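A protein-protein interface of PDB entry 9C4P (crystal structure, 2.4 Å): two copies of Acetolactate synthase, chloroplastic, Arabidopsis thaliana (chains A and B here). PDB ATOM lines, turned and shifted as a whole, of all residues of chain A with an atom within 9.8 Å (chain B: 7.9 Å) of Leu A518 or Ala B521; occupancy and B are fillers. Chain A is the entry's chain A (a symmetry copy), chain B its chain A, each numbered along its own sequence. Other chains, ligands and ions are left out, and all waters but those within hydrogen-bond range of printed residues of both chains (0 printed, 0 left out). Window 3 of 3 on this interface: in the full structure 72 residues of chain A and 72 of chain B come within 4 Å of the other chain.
N of Asn B515 is in hydrogen-bond range of O of Ala A522 (2.8 Å). The backbone carbonyl oxygen (O) of Ala B522 sits at hydrogen-bond distance from the backbone NH (N) of Asn A515, 2.8 Å away.
The backbone NH (N) of Leu B517 sits at hydrogen-bond distance from the side-chain amide oxygen (OD1) of Asn B515 (3.1 Å). OD1 of Asn A515 lies within hydrogen-bond range of N of Leu A517 (3.1 Å). The side-chain amide oxygen of Asn A515 lies within hydrogen-bond range of the guanidinium group of Arg A529, at 3.3 Å.
Cys B523 touches Phe A513 (O to CE1, 3.4 Å). O of Ala B522 touches CB of Pro A514 (3.5 Å). Leu A518 touches Leu B518. CD1 of Leu A518 touches C of Ala B521, 3.7 Å away. Leu A518 touches Ala B522. CB of Ala B522 touches CE2 of Phe A519 (3.8 Å). Phe A519 touches Cys B523. Leu B518 touches Ala A522. CB of Ala A522 touches CE2 of Phe B519, at 3.8 Å. Cys A523 touches Phe B519.
Of the printed residues of chain B, Phe A513 touches Cys B523 (3.4 Å). Leu A518 touches just these residues of chain B: Leu B518 (3.6 Å), Ala B521 (3.7 Å) and Ala B522 (3.6 Å). Of the printed residues of chain B, Ala A521 touches Leu B518. Printed residues of chain B within 4 Å of Cys A523: Phe B519. Of chain A, only Leu A518, Ala A521 and Ala A522 come within 4 Å of Leu B518. No residue of chain A comes within 4 Å of Ala B520. Of chain A, only Leu A518 (3.7 Å) comes within 4 Å of Ala B521. Ala B522 touches just these residues of chain A: Pro A514, Asn A515, Leu A518 and Phe A519. Pro B526 touches none of the printed residues of chain A. The nearest printed residue of chain A that does not touch Asn B515 is Ala A521 (5.0 Å).
Of the 15 printed residues of chain B, 6 touch a printed residue of chain A. Hydrophobic or aromatic side chains of chain B that line the printed part of chain A: Leu B518, Phe B519, Ala B521 and Ala B522. Hydrophobic or aromatic side chains of chain A that line the printed part of chain B: Phe A513, Pro A514, Leu A518, Phe A519, Ala A521 and Ala A522. Among the printed residues, 14 pairs touch across the chains. Among the printed residues, no Asp or Glu carboxylate lies within 4 Å of a Lys or Arg side-chain nitrogen of the other chain.
Leu A518 touches Ala B521, and with the chains exchanged Ala A521 touches Leu B518. Leu A518 touches Ala B522, and with the chains exchanged Ala A522 touches Leu B518. Phe A519 touches Ala B522, and with the chains exchanged Ala A522 touches Phe B519. Phe A519 touches Cys B523, and with the chains exchanged Cys A523 touches Phe B519. Positions printed for both chains: 463, 515, 516, 517, 518, 519, 520, 521, 522, 523, 524, 525, 526, 527 and 551.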
ATOM      1  N   PHE A 456      -4.348  -4.788  27.563  1.00  0.00           N
ATOM      2  CA  PHE A 456      -4.581  -3.570  28.335  1.00  0.00           C
ATOM      3  C   PHE A 456      -5.997  -3.524  28.899  1.00  0.00           C
ATOM      4  O   PHE A 456      -6.207  -3.062  30.027  1.00  0.00           O
ATOM      5  CB  PHE A 456      -4.310  -2.336  27.469  1.00  0.00           C
ATOM      6  CG  PHE A 456      -4.673  -1.036  28.132  1.00  0.00           C
ATOM      7  CD1 PHE A 456      -3.808  -0.440  29.038  1.00  0.00           C
ATOM      8  CD2 PHE A 456      -5.878  -0.407  27.846  1.00  0.00           C
ATOM      9  CE1 PHE A 456      -4.138   0.757  29.653  1.00  0.00           C
ATOM     10  CE2 PHE A 456      -6.214   0.791  28.456  1.00  0.00           C
ATOM     11  CZ  PHE A 456      -5.343   1.375  29.362  1.00  0.00           C
ATOM     12  N   VAL A 460      -7.963  -2.924  32.826  1.00  0.00           N
ATOM     13  CA  VAL A 460      -8.097  -1.490  32.598  1.00  0.00           C
ATOM     14  C   VAL A 460      -8.550  -0.780  33.866  1.00  0.00           C
ATOM     15  O   VAL A 460      -8.293   0.417  34.041  1.00  0.00           O
ATOM     16  CB  VAL A 460      -9.067  -1.235  31.424  1.00  0.00           C
ATOM     17  CG1 VAL A 460     -10.482  -1.639  31.799  1.00  0.00           C
ATOM     18  CG2 VAL A 460      -9.008   0.220  30.978  1.00  0.00           C
ATOM     19  N   LEU A 463      -6.402   1.785  35.991  1.00  0.00           N
ATOM     20  CA  LEU A 463      -6.192   3.202  35.710  1.00  0.00           C
ATOM     21  C   LEU A 463      -6.649   4.059  36.883  1.00  0.00           C
ATOM     22  O   LEU A 463      -6.020   5.076  37.202  1.00  0.00           O
ATOM     23  CB  LEU A 463      -6.931   3.611  34.437  1.00  0.00           C
ATOM     24  CG  LEU A 463      -6.497   2.979  33.115  1.00  0.00           C
ATOM     25  CD1 LEU A 463      -7.458   3.385  32.007  1.00  0.00           C
ATOM     26  CD2 LEU A 463      -5.064   3.372  32.768  1.00  0.00           C
ATOM     27  N   LEU A 477       0.452   2.149  24.231  1.00  0.00           N
ATOM     28  CA  LEU A 477      -0.506   1.136  23.807  1.00  0.00           C
ATOM     29  C   LEU A 477      -0.339   0.887  22.314  1.00  0.00           C
ATOM     30  O   LEU A 477      -0.691   1.738  21.492  1.00  0.00           O
ATOM     31  CB  LEU A 477      -1.928   1.580  24.141  1.00  0.00           C
ATOM     32  CG  LEU A 477      -3.043   0.604  23.777  1.00  0.00           C
ATOM     33  CD1 LEU A 477      -2.720  -0.780  24.294  1.00  0.00           C
ATOM     34  CD2 LEU A 477      -4.343   1.092  24.366  1.00  0.00           C
ATOM     35  N   GLN A 508     -18.925  -1.286  12.990  1.00  0.00           N
ATOM     36  CA  GLN A 508     -18.140  -0.146  12.525  1.00  0.00           C
ATOM     37  C   GLN A 508     -16.691  -0.593  12.351  1.00  0.00           C
ATOM     38  O   GLN A 508     -15.796  -0.223  13.114  1.00  0.00           O
ATOM     39  CB  GLN A 508     -18.275   1.022  13.514  1.00  0.00           C
ATOM     40  CG  GLN A 508     -18.246   0.591  14.974  1.00  0.00           C
ATOM     41  CD  GLN A 508     -18.716   1.679  15.922  1.00  0.00           C
ATOM     42  OE1 GLN A 508     -18.935   2.822  15.516  1.00  0.00           O
ATOM     43  NE2 GLN A 508     -18.880   1.325  17.196  1.00  0.00           N
ATOM     44  N   ILE A 512     -11.661   2.572  15.476  1.00  0.00           N
ATOM     45  CA  ILE A 512     -10.851   2.074  16.584  1.00  0.00           C
ATOM     46  C   ILE A 512     -11.783   1.803  17.761  1.00  0.00           C
ATOM     47  O   ILE A 512     -12.372   2.732  18.322  1.00  0.00           O
ATOM     48  CB  ILE A 512      -9.745   3.064  16.964  1.00  0.00           C
ATOM     49  CG1 ILE A 512      -8.797   3.291  15.783  1.00  0.00           C
ATOM     50  CG2 ILE A 512      -8.980   2.566  18.185  1.00  0.00           C
ATOM     51  CD1 ILE A 512      -8.144   2.022  15.272  1.00  0.00           C
ATOM     52  N   PHE A 513     -11.928   0.531  18.133  1.00  0.00           N
ATOM     53  CA  PHE A 513     -12.806   0.143  19.225  1.00  0.00           C
ATOM     54  C   PHE A 513     -12.076  -0.824  20.150  1.00  0.00           C
ATOM     55  O   PHE A 513     -11.417  -1.764  19.670  1.00  0.00           O
ATOM     56  CB  PHE A 513     -14.098  -0.496  18.704  1.00  0.00           C
ATOM     57  CG  PHE A 513     -15.079  -0.840  19.787  1.00  0.00           C
ATOM     58  CD1 PHE A 513     -16.003   0.095  20.223  1.00  0.00           C
ATOM     59  CD2 PHE A 513     -15.069  -2.096  20.380  1.00  0.00           C
ATOM     60  CE1 PHE A 513     -16.907  -0.215  21.227  1.00  0.00           C
ATOM     61  CE2 PHE A 513     -15.968  -2.412  21.386  1.00  0.00           C
ATOM     62  CZ  PHE A 513     -16.888  -1.469  21.809  1.00  0.00           C
ATOM     63  N   PRO A 514     -12.164  -0.637  21.476  1.00  0.00           N
ATOM     64  CA  PRO A 514     -12.834   0.510  22.098  1.00  0.00           C
ATOM     65  C   PRO A 514     -12.007   1.784  21.986  1.00  0.00           C
ATOM     66  O   PRO A 514     -10.904   1.758  21.439  1.00  0.00           O
ATOM     67  CB  PRO A 514     -12.973   0.090  23.569  1.00  0.00           C
ATOM     68  CG  PRO A 514     -12.741  -1.393  23.584  1.00  0.00           C
ATOM     69  CD  PRO A 514     -11.774  -1.647  22.474  1.00  0.00           C
ATOM     70  N   ASN A 515     -12.542   2.889  22.497  1.00  0.00           N
ATOM     71  CA  ASN A 515     -11.820   4.158  22.524  1.00  0.00           C
ATOM     72  C   ASN A 515     -11.055   4.214  23.839  1.00  0.00           C
ATOM     73  O   ASN A 515     -11.578   4.636  24.872  1.00  0.00           O
ATOM     74  CB  ASN A 515     -12.781   5.328  22.366  1.00  0.00           C
ATOM     75  CG  ASN A 515     -12.067   6.656  22.208  1.00  0.00           C
ATOM     76  OD1 ASN A 515     -10.897   6.798  22.571  1.00  0.00           O
ATOM     77  ND2 ASN A 515     -12.774   7.640  21.670  1.00  0.00           N
ATOM     78  N   MET A 516      -9.794   3.782  23.799  1.00  0.00           N
ATOM     79  CA  MET A 516      -8.987   3.727  25.012  1.00  0.00           C
ATOM     80  C   MET A 516      -8.745   5.104  25.616  1.00  0.00           C
ATOM     81  O   MET A 516      -8.469   5.200  26.817  1.00  0.00           O
ATOM     82  CB  MET A 516      -7.651   3.041  24.719  1.00  0.00           C
ATOM     83  CG  MET A 516      -7.796   1.629  24.171  1.00  0.00           C
ATOM     84  SD  MET A 516      -8.691   0.537  25.290  1.00  0.00           S
ATOM     85  CE  MET A 516      -8.407  -1.048  24.503  1.00  0.00           C
ATOM     86  N   LEU A 517      -8.838   6.168  24.815  1.00  0.00           N
ATOM     87  CA  LEU A 517      -8.675   7.513  25.357  1.00  0.00           C
ATOM     88  C   LEU A 517      -9.748   7.832  26.387  1.00  0.00           C
ATOM     89  O   LEU A 517      -9.479   8.536  27.368  1.00  0.00           O
ATOM     90  CB  LEU A 517      -8.710   8.540  24.228  1.00  0.00           C
ATOM     91  CG  LEU A 517      -7.752   8.284  23.065  1.00  0.00           C
ATOM     92  CD1 LEU A 517      -7.875   9.392  22.031  1.00  0.00           C
ATOM     93  CD2 LEU A 517      -6.324   8.165  23.569  1.00  0.00           C
ATOM     94  N   LEU A 518     -10.965   7.319  26.190  1.00  0.00           N
ATOM     95  CA  LEU A 518     -12.043   7.576  27.136  1.00  0.00           C
ATOM     96  C   LEU A 518     -11.923   6.716  28.389  1.00  0.00           C
ATOM     97  O   LEU A 518     -12.419   7.111  29.449  1.00  0.00           O
ATOM     98  CB  LEU A 518     -13.396   7.362  26.456  1.00  0.00           C
ATOM     99  CG  LEU A 518     -13.648   8.344  25.307  1.00  0.00           C
ATOM    100  CD1 LEU A 518     -14.982   8.082  24.630  1.00  0.00           C
ATOM    101  CD2 LEU A 518     -13.569   9.781  25.807  1.00  0.00           C
ATOM    102  N   PHE A 519     -11.279   5.548  28.293  1.00  0.00           N
ATOM    103  CA  PHE A 519     -10.909   4.818  29.503  1.00  0.00           C
ATOM    104  C   PHE A 519      -9.978   5.658  30.367  1.00  0.00           C
ATOM    105  O   PHE A 519     -10.164   5.762  31.585  1.00  0.00           O
ATOM    106  CB  PHE A 519     -10.244   3.485  29.148  1.00  0.00           C
ATOM    107  CG  PHE A 519     -11.207   2.407  28.740  1.00  0.00           C
ATOM    108  CD1 PHE A 519     -12.161   1.942  29.625  1.00  0.00           C
ATOM    109  CD2 PHE A 519     -11.137   1.836  27.481  1.00  0.00           C
ATOM    110  CE1 PHE A 519     -13.047   0.946  29.258  1.00  0.00           C
ATOM    111  CE2 PHE A 519     -12.019   0.835  27.107  1.00  0.00           C
ATOM    112  CZ  PHE A 519     -12.976   0.392  27.997  1.00  0.00           C
ATOM    113  N   ALA A 520      -8.969   6.274  29.746  1.00  0.00           N
ATOM    114  CA  ALA A 520      -8.062   7.140  30.489  1.00  0.00           C
ATOM    115  C   ALA A 520      -8.781   8.383  30.997  1.00  0.00           C
ATOM    116  O   ALA A 520      -8.549   8.822  32.130  1.00  0.00           O
ATOM    117  CB  ALA A 520      -6.870   7.526  29.612  1.00  0.00           C
ATOM    118  N   ALA A 521      -9.663   8.960  30.174  1.00  0.00           N
ATOM    119  CA  ALA A 521     -10.411  10.139  30.596  1.00  0.00           C
ATOM    120  C   ALA A 521     -11.304   9.827  31.789  1.00  0.00           C
ATOM    121  O   ALA A 521     -11.438  10.648  32.704  1.00  0.00           O
ATOM    122  CB  ALA A 521     -11.241  10.683  29.434  1.00  0.00           C
ATOM    123  N   ALA A 522     -11.916   8.639  31.797  1.00  0.00           N
ATOM    124  CA  ALA A 522     -12.762   8.236  32.917  1.00  0.00           C
ATOM    125  C   ALA A 522     -12.010   8.287  34.238  1.00  0.00           C
ATOM    126  O   ALA A 522     -12.611   8.550  35.286  1.00  0.00           O
ATOM    127  CB  ALA A 522     -13.314   6.831  32.679  1.00  0.00           C
ATOM    128  N   CYS A 523     -10.698   8.048  34.211  1.00  0.00           N
ATOM    129  CA  CYS A 523      -9.876   8.065  35.412  1.00  0.00           C
ATOM    130  C   CYS A 523      -8.989   9.302  35.490  1.00  0.00           C
ATOM    131  O   CYS A 523      -7.971   9.284  36.187  1.00  0.00           O
ATOM    132  CB  CYS A 523      -9.031   6.792  35.489  1.00  0.00           C
ATOM    133  SG  CYS A 523     -10.027   5.275  35.514  1.00  0.00           S
ATOM    134  N   GLY A 524      -9.355  10.374  34.787  1.00  0.00           N
ATOM    135  CA  GLY A 524      -8.614  11.622  34.877  1.00  0.00           C
ATOM    136  C   GLY A 524      -7.168  11.524  34.450  1.00  0.00           C
ATOM    137  O   GLY A 524      -6.313  12.223  35.004  1.00  0.00           O
ATOM    138  N   ILE A 525      -6.870  10.675  33.478  1.00  0.00           N
ATOM    139  CA  ILE A 525      -5.509  10.453  33.001  1.00  0.00           C
ATOM    140  C   ILE A 525      -5.397  11.063  31.609  1.00  0.00           C
ATOM    141  O   ILE A 525      -6.134  10.653  30.700  1.00  0.00           O
ATOM    142  CB  ILE A 525      -5.154   8.957  32.985  1.00  0.00           C
ATOM    143  CG1 ILE A 525      -5.081   8.424  34.418  1.00  0.00           C
ATOM    144  CG2 ILE A 525      -3.850   8.722  32.245  1.00  0.00           C
ATOM    145  CD1 ILE A 525      -4.882   6.931  34.505  1.00  0.00           C
ATOM    146  N   PRO A 526      -4.512  12.038  31.397  1.00  0.00           N
ATOM    147  CA  PRO A 526      -4.374  12.634  30.062  1.00  0.00           C
ATOM    148  C   PRO A 526      -3.941  11.597  29.038  1.00  0.00           C
ATOM    149  O   PRO A 526      -3.160  10.691  29.334  1.00  0.00           O
ATOM    150  CB  PRO A 526      -3.306  13.716  30.261  1.00  0.00           C
ATOM    151  CG  PRO A 526      -2.585  13.327  31.510  1.00  0.00           C
ATOM    152  CD  PRO A 526      -3.600  12.650  32.377  1.00  0.00           C
ATOM    153  N   ALA A 527      -4.462  11.738  27.820  1.00  0.00           N
ATOM    154  CA  ALA A 527      -4.256  10.729  26.793  1.00  0.00           C
ATOM    155  C   ALA A 527      -4.278  11.375  25.417  1.00  0.00           C
ATOM    156  O   ALA A 527      -4.756  12.498  25.239  1.00  0.00           O
ATOM    157  CB  ALA A 527      -5.318   9.626  26.873  1.00  0.00           C
ATOM    158  N   ALA A 528      -3.755  10.639  24.441  1.00  0.00           N
ATOM    159  CA  ALA A 528      -3.765  11.066  23.050  1.00  0.00           C
ATOM    160  C   ALA A 528      -3.622   9.837  22.168  1.00  0.00           C
ATOM    161  O   ALA A 528      -3.138   8.788  22.603  1.00  0.00           O
ATOM    162  CB  ALA A 528      -2.648  12.073  22.755  1.00  0.00           C
ATOM    163  N   ARG A 529      -4.060   9.980  20.921  1.00  0.00           N
ATOM    164  CA  ARG A 529      -3.914   8.950  19.903  1.00  0.00           C
ATOM    165  C   ARG A 529      -3.028   9.476  18.782  1.00  0.00           C
ATOM    166  O   ARG A 529      -3.106  10.652  18.417  1.00  0.00           O
ATOM    167  CB  ARG A 529      -5.279   8.524  19.344  1.00  0.00           C
ATOM    168  CG  ARG A 529      -5.208   7.438  18.278  1.00  0.00           C
ATOM    169  CD  ARG A 529      -6.596   7.037  17.811  1.00  0.00           C
ATOM    170  NE  ARG A 529      -7.411   6.530  18.909  1.00  0.00           N
ATOM    171  CZ  ARG A 529      -8.706   6.261  18.817  1.00  0.00           C
ATOM    172  NH1 ARG A 529      -9.371   6.442  17.688  1.00  0.00           N
ATOM    173  NH2 ARG A 529      -9.351   5.802  19.886  1.00  0.00           N
ATOM    174  N   LEU A 551      -1.524   8.109  28.755  1.00  0.00           N
ATOM    175  CA  LEU A 551      -1.794   7.010  27.835  1.00  0.00           C
ATOM    176  C   LEU A 551      -1.630   7.491  26.399  1.00  0.00           C
ATOM    177  O   LEU A 551      -2.261   8.472  25.994  1.00  0.00           O
ATOM    178  CB  LEU A 551      -3.207   6.455  28.033  1.00  0.00           C
ATOM    179  CG  LEU A 551      -3.761   5.712  26.809  1.00  0.00           C
ATOM    180  CD1 LEU A 551      -3.092   4.359  26.634  1.00  0.00           C
ATOM    181  CD2 LEU A 551      -5.267   5.563  26.875  1.00  0.00           C
ATOM    182  N   ASP A 553      -2.238   6.126  22.701  1.00  0.00           N
ATOM    183  CA  ASP A 553      -2.853   5.112  21.847  1.00  0.00           C
ATOM    184  C   ASP A 553      -2.153   5.150  20.493  1.00  0.00           C
ATOM    185  O   ASP A 553      -2.380   6.056  19.689  1.00  0.00           O
ATOM    186  CB  ASP A 553      -4.350   5.375  21.716  1.00  0.00           C
ATOM    187  CG  ASP A 553      -5.108   4.205  21.113  1.00  0.00           C
ATOM    188  OD1 ASP A 553      -4.591   3.071  21.138  1.00  0.00           O
ATOM    189  OD2 ASP A 553      -6.234   4.425  20.614  1.00  0.00           O
ATOM    190  N   LEU B 463     -17.924  -4.185  28.988  1.00  0.00           N
ATOM    191  CA  LEU B 463     -18.727  -3.235  28.224  1.00  0.00           C
ATOM    192  C   LEU B 463     -18.450  -3.369  26.733  1.00  0.00           C
ATOM    193  O   LEU B 463     -19.365  -3.242  25.909  1.00  0.00           O
ATOM    194  CB  LEU B 463     -18.447  -1.805  28.686  1.00  0.00           C
ATOM    195  CG  LEU B 463     -18.818  -1.424  30.119  1.00  0.00           C
ATOM    196  CD1 LEU B 463     -18.309  -0.024  30.430  1.00  0.00           C
ATOM    197  CD2 LEU B 463     -20.326  -1.517  30.334  1.00  0.00           C
ATOM    198  N   ASN B 515     -15.202   8.380  36.452  1.00  0.00           N
ATOM    199  CA  ASN B 515     -16.352   8.824  35.669  1.00  0.00           C
ATOM    200  C   ASN B 515     -16.832   7.629  34.856  1.00  0.00           C
ATOM    201  O   ASN B 515     -16.348   7.362  33.756  1.00  0.00           O
ATOM    202  CB  ASN B 515     -15.980  10.008  34.787  1.00  0.00           C
ATOM    203  CG  ASN B 515     -17.179  10.619  34.091  1.00  0.00           C
ATOM    204  OD1 ASN B 515     -18.226   9.983  33.945  1.00  0.00           O
ATOM    205  ND2 ASN B 515     -17.028  11.861  33.647  1.00  0.00           N
ATOM    206  N   MET B 516     -17.803   6.901  35.409  1.00  0.00           N
ATOM    207  CA  MET B 516     -18.295   5.696  34.751  1.00  0.00           C
ATOM    208  C   MET B 516     -18.955   5.989  33.410  1.00  0.00           C
ATOM    209  O   MET B 516     -19.031   5.093  32.561  1.00  0.00           O
ATOM    210  CB  MET B 516     -19.277   4.965  35.669  1.00  0.00           C
ATOM    211  CG  MET B 516     -18.681   4.573  37.013  1.00  0.00           C
ATOM    212  SD  MET B 516     -17.244   3.497  36.851  1.00  0.00           S
ATOM    213  CE  MET B 516     -17.008   3.000  38.555  1.00  0.00           C
ATOM    214  N   LEU B 517     -19.436   7.217  33.199  1.00  0.00           N
ATOM    215  CA  LEU B 517     -20.022   7.568  31.910  1.00  0.00           C
ATOM    216  C   LEU B 517     -19.002   7.459  30.787  1.00  0.00           C
ATOM    217  O   LEU B 517     -19.353   7.081  29.663  1.00  0.00           O
ATOM    218  CB  LEU B 517     -20.597   8.981  31.963  1.00  0.00           C
ATOM    219  CG  LEU B 517     -21.562   9.264  33.113  1.00  0.00           C
ATOM    220  CD1 LEU B 517     -22.074  10.693  33.028  1.00  0.00           C
ATOM    221  CD2 LEU B 517     -22.712   8.271  33.100  1.00  0.00           C
ATOM    222  N   LEU B 518     -17.737   7.779  31.070  1.00  0.00           N
ATOM    223  CA  LEU B 518     -16.702   7.695  30.047  1.00  0.00           C
ATOM    224  C   LEU B 518     -16.248   6.260  29.807  1.00  0.00           C
ATOM    225  O   LEU B 518     -15.772   5.946  28.711  1.00  0.00           O
ATOM    226  CB  LEU B 518     -15.517   8.584  30.429  1.00  0.00           C
ATOM    227  CG  LEU B 518     -15.883  10.071  30.489  1.00  0.00           C
ATOM    228  CD1 LEU B 518     -14.697  10.922  30.905  1.00  0.00           C
ATOM    229  CD2 LEU B 518     -16.438  10.538  29.148  1.00  0.00           C
ATOM    230  N   PHE B 519     -16.380   5.382  30.805  1.00  0.00           N
ATOM    231  CA  PHE B 519     -16.211   3.954  30.548  1.00  0.00           C
ATOM    232  C   PHE B 519     -17.231   3.473  29.525  1.00  0.00           C
ATOM    233  O   PHE B 519     -16.891   2.753  28.579  1.00  0.00           O
ATOM    234  CB  PHE B 519     -16.342   3.150  31.844  1.00  0.00           C
ATOM    235  CG  PHE B 519     -15.117   3.182  32.715  1.00  0.00           C
ATOM    236  CD1 PHE B 519     -13.918   2.667  32.262  1.00  0.00           C
ATOM    237  CD2 PHE B 519     -15.174   3.701  33.996  1.00  0.00           C
ATOM    238  CE1 PHE B 519     -12.788   2.688  33.059  1.00  0.00           C
ATOM    239  CE2 PHE B 519     -14.047   3.723  34.802  1.00  0.00           C
ATOM    240  CZ  PHE B 519     -12.853   3.217  34.332  1.00  0.00           C
ATOM    241  N   ALA B 520     -18.493   3.871  29.700  1.00  0.00           N
ATOM    242  CA  ALA B 520     -19.525   3.501  28.737  1.00  0.00           C
ATOM    243  C   ALA B 520     -19.282   4.164  27.388  1.00  0.00           C
ATOM    244  O   ALA B 520     -19.468   3.536  26.337  1.00  0.00           O
ATOM    245  CB  ALA B 520     -20.906   3.870  29.281  1.00  0.00           C
ATOM    246  N   ALA B 521     -18.862   5.434  27.397  1.00  0.00           N
ATOM    247  CA  ALA B 521     -18.585   6.132  26.145  1.00  0.00           C
ATOM    248  C   ALA B 521     -17.447   5.466  25.385  1.00  0.00           C
ATOM    249  O   ALA B 521     -17.492   5.363  24.152  1.00  0.00           O
ATOM    250  CB  ALA B 521     -18.256   7.600  26.422  1.00  0.00           C
ATOM    251  N   ALA B 522     -16.421   5.001  26.105  1.00  0.00           N
ATOM    252  CA  ALA B 522     -15.303   4.315  25.466  1.00  0.00           C
ATOM    253  C   ALA B 522     -15.768   3.117  24.651  1.00  0.00           C
ATOM    254  O   ALA B 522     -15.148   2.777  23.637  1.00  0.00           O
ATOM    255  CB  ALA B 522     -14.288   3.870  26.520  1.00  0.00           C
ATOM    256  N   CYS B 523     -16.859   2.474  25.067  1.00  0.00           N
ATOM    257  CA  CYS B 523     -17.396   1.313  24.370  1.00  0.00           C
ATOM    258  C   CYS B 523     -18.673   1.638  23.604  1.00  0.00           C
ATOM    259  O   CYS B 523     -19.460   0.733  23.314  1.00  0.00           O
ATOM    260  CB  CYS B 523     -17.637   0.172  25.359  1.00  0.00           C
ATOM    261  SG  CYS B 523     -16.132  -0.346  26.231  1.00  0.00           S
ATOM    262  N   GLY B 524     -18.893   2.909  23.273  1.00  0.00           N
ATOM    263  CA  GLY B 524     -20.041   3.289  22.464  1.00  0.00           C
ATOM    264  C   GLY B 524     -21.379   2.957  23.082  1.00  0.00           C
ATOM    265  O   GLY B 524     -22.330   2.639  22.358  1.00  0.00           O
ATOM    266  N   ILE B 525     -21.480   3.017  24.402  1.00  0.00           N
ATOM    267  CA  ILE B 525     -22.701   2.680  25.125  1.00  0.00           C
ATOM    268  C   ILE B 525     -23.289   3.973  25.678  1.00  0.00           C
ATOM    269  O   ILE B 525     -22.622   4.661  26.463  1.00  0.00           O
ATOM    270  CB  ILE B 525     -22.428   1.666  26.248  1.00  0.00           C
ATOM    271  CG1 ILE B 525     -22.030   0.316  25.647  1.00  0.00           C
ATOM    272  CG2 ILE B 525     -23.639   1.528  27.154  1.00  0.00           C
ATOM    273  CD1 ILE B 525     -21.600  -0.706  26.669  1.00  0.00           C
ATOM    274  N   PRO B 526     -24.511   4.346  25.294  1.00  0.00           N
ATOM    275  CA  PRO B 526     -25.106   5.580  25.823  1.00  0.00           C
ATOM    276  C   PRO B 526     -25.263   5.514  27.333  1.00  0.00           C
ATOM    277  O   PRO B 526     -25.555   4.460  27.902  1.00  0.00           O
ATOM    278  CB  PRO B 526     -26.464   5.654  25.113  1.00  0.00           C
ATOM    279  CG  PRO B 526     -26.739   4.262  24.650  1.00  0.00           C
ATOM    280  CD  PRO B 526     -25.404   3.656  24.349  1.00  0.00           C
ATOM    281  N   ALA B 527     -25.064   6.659  27.983  1.00  0.00           N
ATOM    282  CA  ALA B 527     -25.029   6.702  29.437  1.00  0.00           C
ATOM    283  C   ALA B 527     -25.508   8.057  29.930  1.00  0.00           C
ATOM    284  O   ALA B 527     -25.555   9.037  29.181  1.00  0.00           O
ATOM    285  CB  ALA B 527     -23.620   6.416  29.971  1.00  0.00           C
ATOM    286  N   LEU B 551     -26.102   2.689  30.401  1.00  0.00           N
ATOM    287  CA  LEU B 551     -25.584   2.793  31.760  1.00  0.00           C
ATOM    288  C   LEU B 551     -26.174   4.020  32.442  1.00  0.00           C
ATOM    289  O   LEU B 551     -26.068   5.135  31.923  1.00  0.00           O
ATOM    290  CB  LEU B 551     -24.056   2.888  31.765  1.00  0.00           C
ATOM    291  CG  LEU B 551     -23.476   3.528  33.034  1.00  0.00           C
ATOM    292  CD1 LEU B 551     -23.571   2.586  34.222  1.00  0.00           C
ATOM    293  CD2 LEU B 551     -22.049   3.993  32.829  1.00  0.00           C
